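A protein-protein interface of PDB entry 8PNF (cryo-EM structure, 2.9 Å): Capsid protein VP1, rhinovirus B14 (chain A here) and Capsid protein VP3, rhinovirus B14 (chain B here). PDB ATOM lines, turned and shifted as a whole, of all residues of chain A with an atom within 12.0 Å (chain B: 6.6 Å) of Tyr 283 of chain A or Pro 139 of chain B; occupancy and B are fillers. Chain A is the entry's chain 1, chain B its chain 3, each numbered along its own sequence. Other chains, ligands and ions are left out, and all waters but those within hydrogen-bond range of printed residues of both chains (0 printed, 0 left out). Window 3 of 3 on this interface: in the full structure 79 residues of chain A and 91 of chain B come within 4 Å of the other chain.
O of Ser 282 of chain A sits close to O of Gly 82 of chain B, 3.0 Å away.
The backbone carbonyl oxygen (O) of Pro 139 of chain B sits close to the side-chain hydroxyl (OH) of Tyr 283 of chain A (2.3 Å).
The guanidinium group (NH1) of Arg 276 of chain A lies within hydrogen-bond range of the backbone carbonyl oxygen (O) of Gly 82 of chain B, 2.9 Å away.
The side-chain hydroxyl (OH) of Tyr 283 of chain A is in hydrogen-bond range of the side-chain amide nitrogen (NE2) of Gln 79 of chain B.
O of Lys 281 of chain A sits at hydrogen-bond distance from NE2 of Gln 79 of chain B, 3.2 Å away.
N of Gly 82 of chain B is in hydrogen-bond range of O of Ile 280 of chain A (3.3 Å).
The side-chain hydroxyl (OG) of Ser 282 of chain A lies within hydrogen-bond range of the backbone carbonyl oxygen (O) of Asp 279 of chain A.
The backbone NH (N) of Thr 132 of chain B sits at hydrogen-bond distance from the backbone carbonyl oxygen (O) of Phe 186 of chain B.
OG of Ser 188 of chain B is in hydrogen-bond range of NE1 of Trp 190 of chain B (2.9 Å).
The backbone NH of Ala 130 of chain B is in hydrogen-bond range of the backbone carbonyl oxygen of Ser 188 of chain B (2.9 Å).
The backbone carbonyl oxygen (O) of Phe 81 of chain B is in hydrogen-bond range of the side-chain amide nitrogen (NE2) of Gln 79 of chain B, 3.0 Å away.
The guanidinium group (NH1) of Arg 276 of chain A is in hydrogen-bond range of the backbone carbonyl oxygen (O) of Ser 282 of chain A (2.6 Å).
Among the printed residues, merely in contact across the chains: Arg 276 of chain A with Thr 83 of chain B, Lys 281 of chain A with Gly 82 of chain B, Tyr 283 of chain A with Gly 82 of chain B, Tyr 283 of chain A with Thr 83 of chain B, Tyr 283 of chain A with Gly 138 of chain B, Tyr 283 of chain A with Phe 186 of chain B, Tyr 283 of chain A with Leu 187 of chain B, Tyr 283 of chain A with Ser 188 of chain B and Tyr 283 of chain A with Trp 190 of chain B.
Pro 139 of chain B touches just one residue of chain A: Tyr 283.
Gly 82 of chain B touches five residues of chain A.
Of the printed residues of chain A, Thr 83 of chain B touches Arg 276 and Tyr 283.
No residue of chain A comes within 4 Å of Ala 130 of chain B.
Thr 132 of chain B touches none of the printed residues of chain A.
Arg 137 of chain B touches none of the printed residues of chain A.
Gly 138 of chain B touches just one residue of chain A: Tyr 283 (3.7 Å).
No residue of chain A comes within 4 Å of Gln 140 of chain B.
No residue of chain A comes within 4 Å of Asp 141 of chain B.
No residue of chain A comes within 4 Å of Glu 144 of chain B.
Of chain A, only Tyr 283 (3.6 Å) comes within 4 Å of Phe 186 of chain B.
Of the printed residues of chain B, Ile 280 of chain A touches Gly 82.
Printed residues of chain A within 4 Å of Gln 79 of chain B: Lys 281 (3.2 Å) and Tyr 283 (3.2 Å).
Of the printed residues of chain A, Leu 187 of chain B touches Tyr 283 (3.8 Å).
Printed residues of chain B within 4 Å of Lys 281 of chain A: Gln 79 (3.2 Å) and Gly 82 (3.7 Å).
Of the printed residues of chain B, Ser 282 of chain A touches Gly 82 (3.0 Å).
The nearest residue of chain B that does not touch Tyr 283 of chain A is Asn 84 of chain B (4.1 Å).
The nearest residue of chain A that does not touch Pro 139 of chain B is Lys 281 of chain A (6.0 Å).
The nearest printed residue of chain B that does not touch Arg 276 of chain A is Phe 81 of chain B (5.6 Å).
Along chain B the printed residues that touch a printed residue of chain A span positions 79 to 190.
Of the 10 printed residues of chain A, 5 touch a printed residue of chain B.
Hydrophobic or aromatic side chains of chain A that line the printed part of chain B: Tyr 283.
Among the printed residues, no Asp or Glu carboxylate lies within 4 Å of a Lys or Arg side-chain nitrogen of the other chain.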
ATOM      1  N   LYS A 274       6.862 -10.788  -8.633  1.00  0.00           N
ATOM      2  CA  LYS A 274       6.189 -11.773  -7.801  1.00  0.00           C
ATOM      3  C   LYS A 274       6.306 -13.150  -8.435  1.00  0.00           C
ATOM      4  O   LYS A 274       5.967 -13.332  -9.607  1.00  0.00           O
ATOM      5  CB  LYS A 274       4.728 -11.384  -7.617  1.00  0.00           C
ATOM      6  CG  LYS A 274       4.551 -10.097  -6.844  1.00  0.00           C
ATOM      7  CD  LYS A 274       3.110  -9.655  -6.842  1.00  0.00           C
ATOM      8  CE  LYS A 274       2.276 -10.501  -5.902  1.00  0.00           C
ATOM      9  NZ  LYS A 274       0.963 -10.834  -6.515  1.00  0.00           N
ATOM     10  N   LYS A 275       6.791 -14.114  -7.663  1.00  0.00           N
ATOM     11  CA  LYS A 275       6.871 -15.481  -8.150  1.00  0.00           C
ATOM     12  C   LYS A 275       5.477 -16.089  -8.193  1.00  0.00           C
ATOM     13  O   LYS A 275       4.658 -15.860  -7.299  1.00  0.00           O
ATOM     14  CB  LYS A 275       7.797 -16.309  -7.256  1.00  0.00           C
ATOM     15  CG  LYS A 275       8.121 -17.678  -7.797  1.00  0.00           C
ATOM     16  CD  LYS A 275       9.108 -18.420  -6.929  1.00  0.00           C
ATOM     17  CE  LYS A 275       9.346 -19.816  -7.469  1.00  0.00           C
ATOM     18  NZ  LYS A 275      10.277 -20.596  -6.618  1.00  0.00           N
ATOM     19  N   ARG A 276       5.202 -16.840  -9.255  1.00  0.00           N
ATOM     20  CA  ARG A 276       3.910 -17.492  -9.400  1.00  0.00           C
ATOM     21  C   ARG A 276       3.747 -18.596  -8.368  1.00  0.00           C
ATOM     22  O   ARG A 276       4.678 -19.356  -8.094  1.00  0.00           O
ATOM     23  CB  ARG A 276       3.766 -18.085 -10.799  1.00  0.00           C
ATOM     24  CG  ARG A 276       2.972 -17.254 -11.776  1.00  0.00           C
ATOM     25  CD  ARG A 276       3.310 -17.691 -13.181  1.00  0.00           C
ATOM     26  NE  ARG A 276       2.848 -16.766 -14.204  1.00  0.00           N
ATOM     27  CZ  ARG A 276       1.676 -16.866 -14.816  1.00  0.00           C
ATOM     28  NH1 ARG A 276       0.843 -17.841 -14.498  1.00  0.00           N
ATOM     29  NH2 ARG A 276       1.336 -15.986 -15.740  1.00  0.00           N
ATOM     30  N   LYS A 277       2.552 -18.681  -7.793  1.00  0.00           N
ATOM     31  CA  LYS A 277       2.197 -19.795  -6.917  1.00  0.00           C
ATOM     32  C   LYS A 277       1.669 -20.965  -7.749  1.00  0.00           C
ATOM     33  O   LYS A 277       0.495 -21.323  -7.721  1.00  0.00           O
ATOM     34  CB  LYS A 277       1.191 -19.339  -5.865  1.00  0.00           C
ATOM     35  CG  LYS A 277       1.654 -18.211  -4.910  1.00  0.00           C
ATOM     36  CD  LYS A 277       2.729 -18.631  -3.871  1.00  0.00           C
ATOM     37  CE  LYS A 277       4.187 -18.367  -4.291  1.00  0.00           C
ATOM     38  NZ  LYS A 277       5.156 -18.696  -3.210  1.00  0.00           N
ATOM     39  N   GLY A 278       2.576 -21.547  -8.503  1.00  0.00           N
ATOM     40  CA  GLY A 278       2.250 -22.580  -9.451  1.00  0.00           C
ATOM     41  C   GLY A 278       3.215 -22.523 -10.627  1.00  0.00           C
ATOM     42  O   GLY A 278       4.385 -22.170 -10.465  1.00  0.00           O
ATOM     43  N   ASP A 279       2.706 -22.885 -11.796  1.00  0.00           N
ATOM     44  CA  ASP A 279       3.486 -22.850 -13.018  1.00  0.00           C
ATOM     45  C   ASP A 279       3.053 -21.665 -13.880  1.00  0.00           C
ATOM     46  O   ASP A 279       2.284 -20.804 -13.451  1.00  0.00           O
ATOM     47  CB  ASP A 279       3.356 -24.178 -13.752  1.00  0.00           C
ATOM     48  CG  ASP A 279       2.008 -24.352 -14.390  1.00  0.00           C
ATOM     49  OD1 ASP A 279       1.905 -24.088 -15.596  1.00  0.00           O
ATOM     50  OD2 ASP A 279       1.055 -24.745 -13.689  1.00  0.00           O
ATOM     51  N   ILE A 280       3.562 -21.613 -15.113  1.00  0.00           N
ATOM     52  CA  ILE A 280       3.322 -20.458 -15.973  1.00  0.00           C
ATOM     53  C   ILE A 280       1.894 -20.467 -16.521  1.00  0.00           C
ATOM     54  O   ILE A 280       1.305 -19.406 -16.757  1.00  0.00           O
ATOM     55  CB  ILE A 280       4.394 -20.418 -17.086  1.00  0.00           C
ATOM     56  CG1 ILE A 280       4.253 -19.178 -17.976  1.00  0.00           C
ATOM     57  CG2 ILE A 280       4.386 -21.697 -17.908  1.00  0.00           C
ATOM     58  CD1 ILE A 280       5.400 -18.965 -18.933  1.00  0.00           C
ATOM     59  N   LYS A 281       1.284 -21.645 -16.659  1.00  0.00           N
ATOM     60  CA  LYS A 281      -0.045 -21.778 -17.245  1.00  0.00           C
ATOM     61  C   LYS A 281      -1.159 -21.558 -16.231  1.00  0.00           C
ATOM     62  O   LYS A 281      -2.326 -21.846 -16.524  1.00  0.00           O
ATOM     63  CB  LYS A 281      -0.190 -23.155 -17.895  1.00  0.00           C
ATOM     64  CG  LYS A 281       1.015 -23.584 -18.711  1.00  0.00           C
ATOM     65  CD  LYS A 281       0.863 -24.999 -19.234  1.00  0.00           C
ATOM     66  CE  LYS A 281       0.885 -26.023 -18.119  1.00  0.00           C
ATOM     67  NZ  LYS A 281       2.217 -26.104 -17.468  1.00  0.00           N
ATOM     68  N   SER A 282      -0.836 -21.044 -15.051  1.00  0.00           N
ATOM     69  CA  SER A 282      -1.778 -20.939 -13.950  1.00  0.00           C
ATOM     70  C   SER A 282      -2.320 -19.522 -13.852  1.00  0.00           C
ATOM     71  O   SER A 282      -1.558 -18.551 -13.875  1.00  0.00           O
ATOM     72  CB  SER A 282      -1.114 -21.339 -12.637  1.00  0.00           C
ATOM     73  OG  SER A 282       0.053 -20.574 -12.419  1.00  0.00           O
ATOM     74  N   TYR A 283      -3.634 -19.413 -13.725  1.00  0.00           N
ATOM     75  CA  TYR A 283      -4.305 -18.123 -13.690  1.00  0.00           C
ATOM     76  C   TYR A 283      -4.266 -17.517 -12.299  1.00  0.00           C
ATOM     77  O   TYR A 283      -5.176 -17.724 -11.500  1.00  0.00           O
ATOM     78  CB  TYR A 283      -5.754 -18.269 -14.157  1.00  0.00           C
ATOM     79  CG  TYR A 283      -5.893 -18.986 -15.476  1.00  0.00           C
ATOM     80  CD1 TYR A 283      -5.738 -18.306 -16.676  1.00  0.00           C
ATOM     81  CD2 TYR A 283      -6.182 -20.340 -15.521  1.00  0.00           C
ATOM     82  CE1 TYR A 283      -5.858 -18.960 -17.880  1.00  0.00           C
ATOM     83  CE2 TYR A 283      -6.301 -20.999 -16.714  1.00  0.00           C
ATOM     84  CZ  TYR A 283      -6.142 -20.305 -17.892  1.00  0.00           C
ATOM     85  OH  TYR A 283      -6.265 -20.966 -19.089  1.00  0.00           O
ATOM     86  N   GLN B  79      -0.921 -25.876 -23.543  1.00  0.00           N
ATOM     87  CA  GLN B  79      -1.036 -24.484 -23.136  1.00  0.00           C
ATOM     88  C   GLN B  79       0.346 -23.854 -23.088  1.00  0.00           C
ATOM     89  O   GLN B  79       1.294 -24.464 -22.587  1.00  0.00           O
ATOM     90  CB  GLN B  79      -1.704 -24.373 -21.772  1.00  0.00           C
ATOM     91  CG  GLN B  79      -2.184 -22.994 -21.420  1.00  0.00           C
ATOM     92  CD  GLN B  79      -2.918 -22.967 -20.107  1.00  0.00           C
ATOM     93  OE1 GLN B  79      -3.223 -24.008 -19.534  1.00  0.00           O
ATOM     94  NE2 GLN B  79      -3.214 -21.772 -19.623  1.00  0.00           N
ATOM     95  N   PHE B  81       0.847 -20.243 -22.067  1.00  0.00           N
ATOM     96  CA  PHE B  81       0.824 -19.484 -20.823  1.00  0.00           C
ATOM     97  C   PHE B  81      -0.619 -19.297 -20.372  1.00  0.00           C
ATOM     98  O   PHE B  81      -1.569 -19.660 -21.069  1.00  0.00           O
ATOM     99  CB  PHE B  81       1.566 -18.142 -20.953  1.00  0.00           C
ATOM    100  CG  PHE B  81       1.102 -17.246 -22.089  1.00  0.00           C
ATOM    101  CD1 PHE B  81      -0.055 -16.476 -21.995  1.00  0.00           C
ATOM    102  CD2 PHE B  81       1.879 -17.115 -23.218  1.00  0.00           C
ATOM    103  CE1 PHE B  81      -0.437 -15.637 -23.012  1.00  0.00           C
ATOM    104  CE2 PHE B  81       1.503 -16.273 -24.237  1.00  0.00           C
ATOM    105  CZ  PHE B  81       0.348 -15.529 -24.131  1.00  0.00           C
ATOM    106  N   GLY B  82      -0.769 -18.690 -19.200  1.00  0.00           N
ATOM    107  CA  GLY B  82      -2.061 -18.313 -18.672  1.00  0.00           C
ATOM    108  C   GLY B  82      -1.925 -17.390 -17.481  1.00  0.00           C
ATOM    109  O   GLY B  82      -1.057 -17.601 -16.630  1.00  0.00           O
ATOM    110  N   THR B  83      -2.762 -16.361 -17.408  1.00  0.00           N
ATOM    111  CA  THR B  83      -2.733 -15.443 -16.281  1.00  0.00           C
ATOM    112  C   THR B  83      -4.104 -14.809 -16.116  1.00  0.00           C
ATOM    113  O   THR B  83      -4.952 -14.883 -17.009  1.00  0.00           O
ATOM    114  CB  THR B  83      -1.659 -14.357 -16.455  1.00  0.00           C
ATOM    115  OG1 THR B  83      -1.477 -13.651 -15.222  1.00  0.00           O
ATOM    116  CG2 THR B  83      -2.042 -13.376 -17.544  1.00  0.00           C
ATOM    117  N   ASN B  84      -4.323 -14.218 -14.950  1.00  0.00           N
ATOM    118  CA  ASN B  84      -5.474 -13.363 -14.738  1.00  0.00           C
ATOM    119  C   ASN B  84      -5.133 -11.942 -15.163  1.00  0.00           C
ATOM    120  O   ASN B  84      -3.968 -11.571 -15.303  1.00  0.00           O
ATOM    121  CB  ASN B  84      -5.901 -13.389 -13.276  1.00  0.00           C
ATOM    122  CG  ASN B  84      -4.752 -13.127 -12.345  1.00  0.00           C
ATOM    123  OD1 ASN B  84      -3.596 -13.302 -12.711  1.00  0.00           O
ATOM    124  ND2 ASN B  84      -5.058 -12.706 -11.135  1.00  0.00           N
ATOM    125  N   ALA B 130      -6.257 -16.292 -26.422  1.00  0.00           N
ATOM    126  CA  ALA B 130      -7.657 -16.136 -26.066  1.00  0.00           C
ATOM    127  C   ALA B 130      -7.815 -15.290 -24.814  1.00  0.00           C
ATOM    128  O   ALA B 130      -7.012 -15.390 -23.882  1.00  0.00           O
ATOM    129  CB  ALA B 130      -8.309 -17.494 -25.861  1.00  0.00           C
ATOM    130  N   THR B 132     -10.634 -14.582 -21.868  1.00  0.00           N
ATOM    131  CA  THR B 132     -11.865 -15.047 -21.252  1.00  0.00           C
ATOM    132  C   THR B 132     -12.517 -13.897 -20.504  1.00  0.00           C
ATOM    133  O   THR B 132     -11.929 -13.392 -19.544  1.00  0.00           O
ATOM    134  CB  THR B 132     -11.583 -16.194 -20.298  1.00  0.00           C
ATOM    135  OG1 THR B 132     -10.782 -17.175 -20.964  1.00  0.00           O
ATOM    136  CG2 THR B 132     -12.870 -16.835 -19.821  1.00  0.00           C
ATOM    137  N   ARG B 137     -14.623 -19.329 -15.452  1.00  0.00           N
ATOM    138  CA  ARG B 137     -13.336 -19.653 -14.863  1.00  0.00           C
ATOM    139  C   ARG B 137     -12.225 -19.488 -15.896  1.00  0.00           C
ATOM    140  O   ARG B 137     -12.466 -19.186 -17.066  1.00  0.00           O
ATOM    141  CB  ARG B 137     -13.349 -21.076 -14.317  1.00  0.00           C
ATOM    142  CG  ARG B 137     -13.506 -22.133 -15.393  1.00  0.00           C
ATOM    143  CD  ARG B 137     -13.222 -23.518 -14.849  1.00  0.00           C
ATOM    144  NE  ARG B 137     -12.899 -24.464 -15.908  1.00  0.00           N
ATOM    145  CZ  ARG B 137     -13.461 -25.660 -16.045  1.00  0.00           C
ATOM    146  NH1 ARG B 137     -14.382 -26.067 -15.186  1.00  0.00           N
ATOM    147  NH2 ARG B 137     -13.099 -26.451 -17.042  1.00  0.00           N
ATOM    148  N   GLY B 138     -10.986 -19.685 -15.456  1.00  0.00           N
ATOM    149  CA  GLY B 138      -9.867 -19.776 -16.360  1.00  0.00           C
ATOM    150  C   GLY B 138      -9.944 -21.053 -17.170  1.00  0.00           C
ATOM    151  O   GLY B 138     -10.173 -22.136 -16.627  1.00  0.00           O
ATOM    152  N   PRO B 139      -9.776 -20.946 -18.490  1.00  0.00           N
ATOM    153  CA  PRO B 139      -9.963 -22.114 -19.365  1.00  0.00           C
ATOM    154  C   PRO B 139      -8.869 -23.153 -19.171  1.00  0.00           C
ATOM    155  O   PRO B 139      -7.695 -22.817 -19.012  1.00  0.00           O
ATOM    156  CB  PRO B 139      -9.924 -21.511 -20.772  1.00  0.00           C
ATOM    157  CG  PRO B 139      -9.193 -20.244 -20.622  1.00  0.00           C
ATOM    158  CD  PRO B 139      -9.495 -19.723 -19.257  1.00  0.00           C
ATOM    159  N   GLN B 140      -9.270 -24.423 -19.173  1.00  0.00           N
ATOM    160  CA  GLN B 140      -8.373 -25.519 -18.847  1.00  0.00           C
ATOM    161  C   GLN B 140      -8.056 -26.416 -20.036  1.00  0.00           C
ATOM    162  O   GLN B 140      -7.137 -27.236 -19.945  1.00  0.00           O
ATOM    163  CB  GLN B 140      -8.962 -26.355 -17.709  1.00  0.00           C
ATOM    164  CG  GLN B 140      -9.529 -25.512 -16.585  1.00  0.00           C
ATOM    165  CD  GLN B 140      -9.854 -26.318 -15.352  1.00  0.00           C
ATOM    166  OE1 GLN B 140      -9.976 -27.540 -15.406  1.00  0.00           O
ATOM    167  NE2 GLN B 140     -10.009 -25.634 -14.228  1.00  0.00           N
ATOM    168  N   ASP B 141      -8.785 -26.286 -21.138  1.00  0.00           N
ATOM    169  CA  ASP B 141      -8.377 -26.866 -22.404  1.00  0.00           C
ATOM    170  C   ASP B 141      -8.580 -25.832 -23.503  1.00  0.00           C
ATOM    171  O   ASP B 141      -9.114 -24.746 -23.267  1.00  0.00           O
ATOM    172  CB  ASP B 141      -9.090 -28.203 -22.680  1.00  0.00           C
ATOM    173  CG  ASP B 141     -10.608 -28.087 -22.800  1.00  0.00           C
ATOM    174  OD1 ASP B 141     -11.201 -27.005 -22.638  1.00  0.00           O
ATOM    175  OD2 ASP B 141     -11.227 -29.132 -23.068  1.00  0.00           O
ATOM    176  N   ARG B 142      -8.117 -26.164 -24.707  1.00  0.00           N
ATOM    177  CA  ARG B 142      -8.192 -25.230 -25.824  1.00  0.00           C
ATOM    178  C   ARG B 142      -9.618 -24.959 -26.273  1.00  0.00           C
ATOM    179  O   ARG B 142      -9.899 -23.854 -26.743  1.00  0.00           O
ATOM    180  CB  ARG B 142      -7.378 -25.750 -27.003  1.00  0.00           C
ATOM    181  CG  ARG B 142      -6.960 -24.677 -27.979  1.00  0.00           C
ATOM    182  CD  ARG B 142      -6.327 -25.271 -29.208  1.00  0.00           C
ATOM    183  NE  ARG B 142      -7.271 -26.059 -29.984  1.00  0.00           N
ATOM    184  CZ  ARG B 142      -6.919 -26.924 -30.926  1.00  0.00           C
ATOM    185  NH1 ARG B 142      -5.643 -27.109 -31.215  1.00  0.00           N
ATOM    186  NH2 ARG B 142      -7.846 -27.598 -31.583  1.00  0.00           N
ATOM    187  N   ARG B 143     -10.517 -25.934 -26.144  1.00  0.00           N
ATOM    188  CA  ARG B 143     -11.898 -25.727 -26.559  1.00  0.00           C
ATOM    189  C   ARG B 143     -12.615 -24.739 -25.646  1.00  0.00           C
ATOM    190  O   ARG B 143     -13.493 -24.003 -26.106  1.00  0.00           O
ATOM    191  CB  ARG B 143     -12.628 -27.069 -26.603  1.00  0.00           C
ATOM    192  CG  ARG B 143     -14.029 -26.998 -27.164  1.00  0.00           C
ATOM    193  CD  ARG B 143     -14.869 -28.169 -26.741  1.00  0.00           C
ATOM    194  NE  ARG B 143     -16.254 -27.760 -26.554  1.00  0.00           N
ATOM    195  CZ  ARG B 143     -17.255 -28.123 -27.345  1.00  0.00           C
ATOM    196  NH1 ARG B 143     -17.028 -28.902 -28.393  1.00  0.00           N
ATOM    197  NH2 ARG B 143     -18.483 -27.700 -27.094  1.00  0.00           N
ATOM    198  N   GLU B 144     -12.257 -24.709 -24.359  1.00  0.00           N
ATOM    199  CA  GLU B 144     -12.829 -23.728 -23.441  1.00  0.00           C
ATOM    200  C   GLU B 144     -12.425 -22.311 -23.817  1.00  0.00           C
ATOM    201  O   GLU B 144     -13.271 -21.414 -23.879  1.00  0.00           O
ATOM    202  CB  GLU B 144     -12.399 -24.035 -22.011  1.00  0.00           C
ATOM    203  CG  GLU B 144     -13.433 -23.694 -20.971  1.00  0.00           C
ATOM    204  CD  GLU B 144     -13.073 -24.223 -19.604  1.00  0.00           C
ATOM    205  OE1 GLU B 144     -12.048 -24.919 -19.486  1.00  0.00           O
ATOM    206  OE2 GLU B 144     -13.813 -23.937 -18.644  1.00  0.00           O
ATOM    207  N   ALA B 145     -11.141 -22.098 -24.096  1.00  0.00           N
ATOM    208  CA  ALA B 145     -10.663 -20.782 -24.490  1.00  0.00           C
ATOM    209  C   ALA B 145     -11.086 -20.412 -25.901  1.00  0.00           C
ATOM    210  O   ALA B 145     -11.124 -19.225 -26.235  1.00  0.00           O
ATOM    211  CB  ALA B 145      -9.149 -20.738 -24.372  1.00  0.00           C
ATOM    212  N   MET B 146     -11.419 -21.406 -26.721  1.00  0.00           N
ATOM    213  CA  MET B 146     -11.880 -21.179 -28.086  1.00  0.00           C
ATOM    214  C   MET B 146     -13.226 -20.460 -28.125  1.00  0.00           C
ATOM    215  O   MET B 146     -13.548 -19.802 -29.119  1.00  0.00           O
ATOM    216  CB  MET B 146     -11.910 -22.544 -28.787  1.00  0.00           C
ATOM    217  CG  MET B 146     -12.300 -22.642 -30.251  1.00  0.00           C
ATOM    218  SD  MET B 146     -14.068 -22.664 -30.565  1.00  0.00           S
ATOM    219  CE  MET B 146     -14.454 -24.302 -29.970  1.00  0.00           C
ATOM    220  N   PHE B 186      -9.425 -13.442 -17.845  1.00  0.00           N
ATOM    221  CA  PHE B 186      -8.276 -14.325 -17.944  1.00  0.00           C
ATOM    222  C   PHE B 186      -7.704 -14.255 -19.353  1.00  0.00           C
ATOM    223  O   PHE B 186      -8.393 -13.899 -20.310  1.00  0.00           O
ATOM    224  CB  PHE B 186      -8.656 -15.766 -17.577  1.00  0.00           C
ATOM    225  CG  PHE B 186      -9.235 -15.897 -16.203  1.00  0.00           C
ATOM    226  CD1 PHE B 186      -8.410 -16.019 -15.102  1.00  0.00           C
ATOM    227  CD2 PHE B 186     -10.605 -15.865 -16.007  1.00  0.00           C
ATOM    228  CE1 PHE B 186      -8.936 -16.127 -13.834  1.00  0.00           C
ATOM    229  CE2 PHE B 186     -11.138 -15.967 -14.740  1.00  0.00           C
ATOM    230  CZ  PHE B 186     -10.301 -16.098 -13.653  1.00  0.00           C
ATOM    231  N   LEU B 187      -6.418 -14.579 -19.462  1.00  0.00           N
ATOM    232  CA  LEU B 187      -5.682 -14.523 -20.718  1.00  0.00           C
ATOM    233  C   LEU B 187      -4.844 -15.786 -20.820  1.00  0.00           C
ATOM    234  O   LEU B 187      -4.219 -16.180 -19.837  1.00  0.00           O
ATOM    235  CB  LEU B 187      -4.783 -13.284 -20.768  1.00  0.00           C
ATOM    236  CG  LEU B 187      -3.947 -13.010 -22.017  1.00  0.00           C
ATOM    237  CD1 LEU B 187      -4.752 -12.210 -22.991  1.00  0.00           C
ATOM    238  CD2 LEU B 187      -2.671 -12.276 -21.669  1.00  0.00           C
ATOM    239  N   SER B 188      -4.839 -16.424 -21.988  1.00  0.00           N
ATOM    240  CA  SER B 188      -4.075 -17.651 -22.165  1.00  0.00           C
ATOM    241  C   SER B 188      -3.698 -17.817 -23.627  1.00  0.00           C
ATOM    242  O   SER B 188      -4.243 -17.151 -24.509  1.00  0.00           O
ATOM    243  CB  SER B 188      -4.853 -18.878 -21.685  1.00  0.00           C
ATOM    244  OG  SER B 188      -6.040 -19.055 -22.435  1.00  0.00           O
ATOM    245  N   CYS B 189      -2.743 -18.711 -23.870  1.00  0.00           N
ATOM    246  CA  CYS B 189      -2.337 -19.068 -25.221  1.00  0.00           C
ATOM    247  C   CYS B 189      -2.164 -20.573 -25.312  1.00  0.00           C
ATOM    248  O   CYS B 189      -1.746 -21.221 -24.351  1.00  0.00           O
ATOM    249  CB  CYS B 189      -1.041 -18.374 -25.632  1.00  0.00           C
ATOM    250  SG  CYS B 189      -0.443 -18.736 -27.284  1.00  0.00           S
ATOM    251  N   TRP B 190      -2.494 -21.117 -26.474  1.00  0.00           N
ATOM    252  CA  TRP B 190      -2.504 -22.550 -26.697  1.00  0.00           C
ATOM    253  C   TRP B 190      -1.893 -22.837 -28.057  1.00  0.00           C
ATOM    254  O   TRP B 190      -1.808 -21.960 -28.917  1.00  0.00           O
ATOM    255  CB  TRP B 190      -3.932 -23.129 -26.631  1.00  0.00           C
ATOM    256  CG  TRP B 190      -4.717 -22.720 -25.427  1.00  0.00           C
ATOM    257  CD1 TRP B 190      -5.333 -21.523 -25.211  1.00  0.00           C
ATOM    258  CD2 TRP B 190      -4.961 -23.508 -24.263  1.00  0.00           C
ATOM    259  NE1 TRP B 190      -5.928 -21.513 -23.983  1.00  0.00           N
ATOM    260  CE2 TRP B 190      -5.721 -22.724 -23.382  1.00  0.00           C
ATOM    261  CE3 TRP B 190      -4.614 -24.804 -23.882  1.00  0.00           C
ATOM    262  CZ2 TRP B 190      -6.139 -23.191 -22.148  1.00  0.00           C
ATOM    263  CZ3 TRP B 190      -5.028 -25.262 -22.659  1.00  0.00           C
ATOM    264  CH2 TRP B 190      -5.781 -24.460 -21.805  1.00  0.00           C
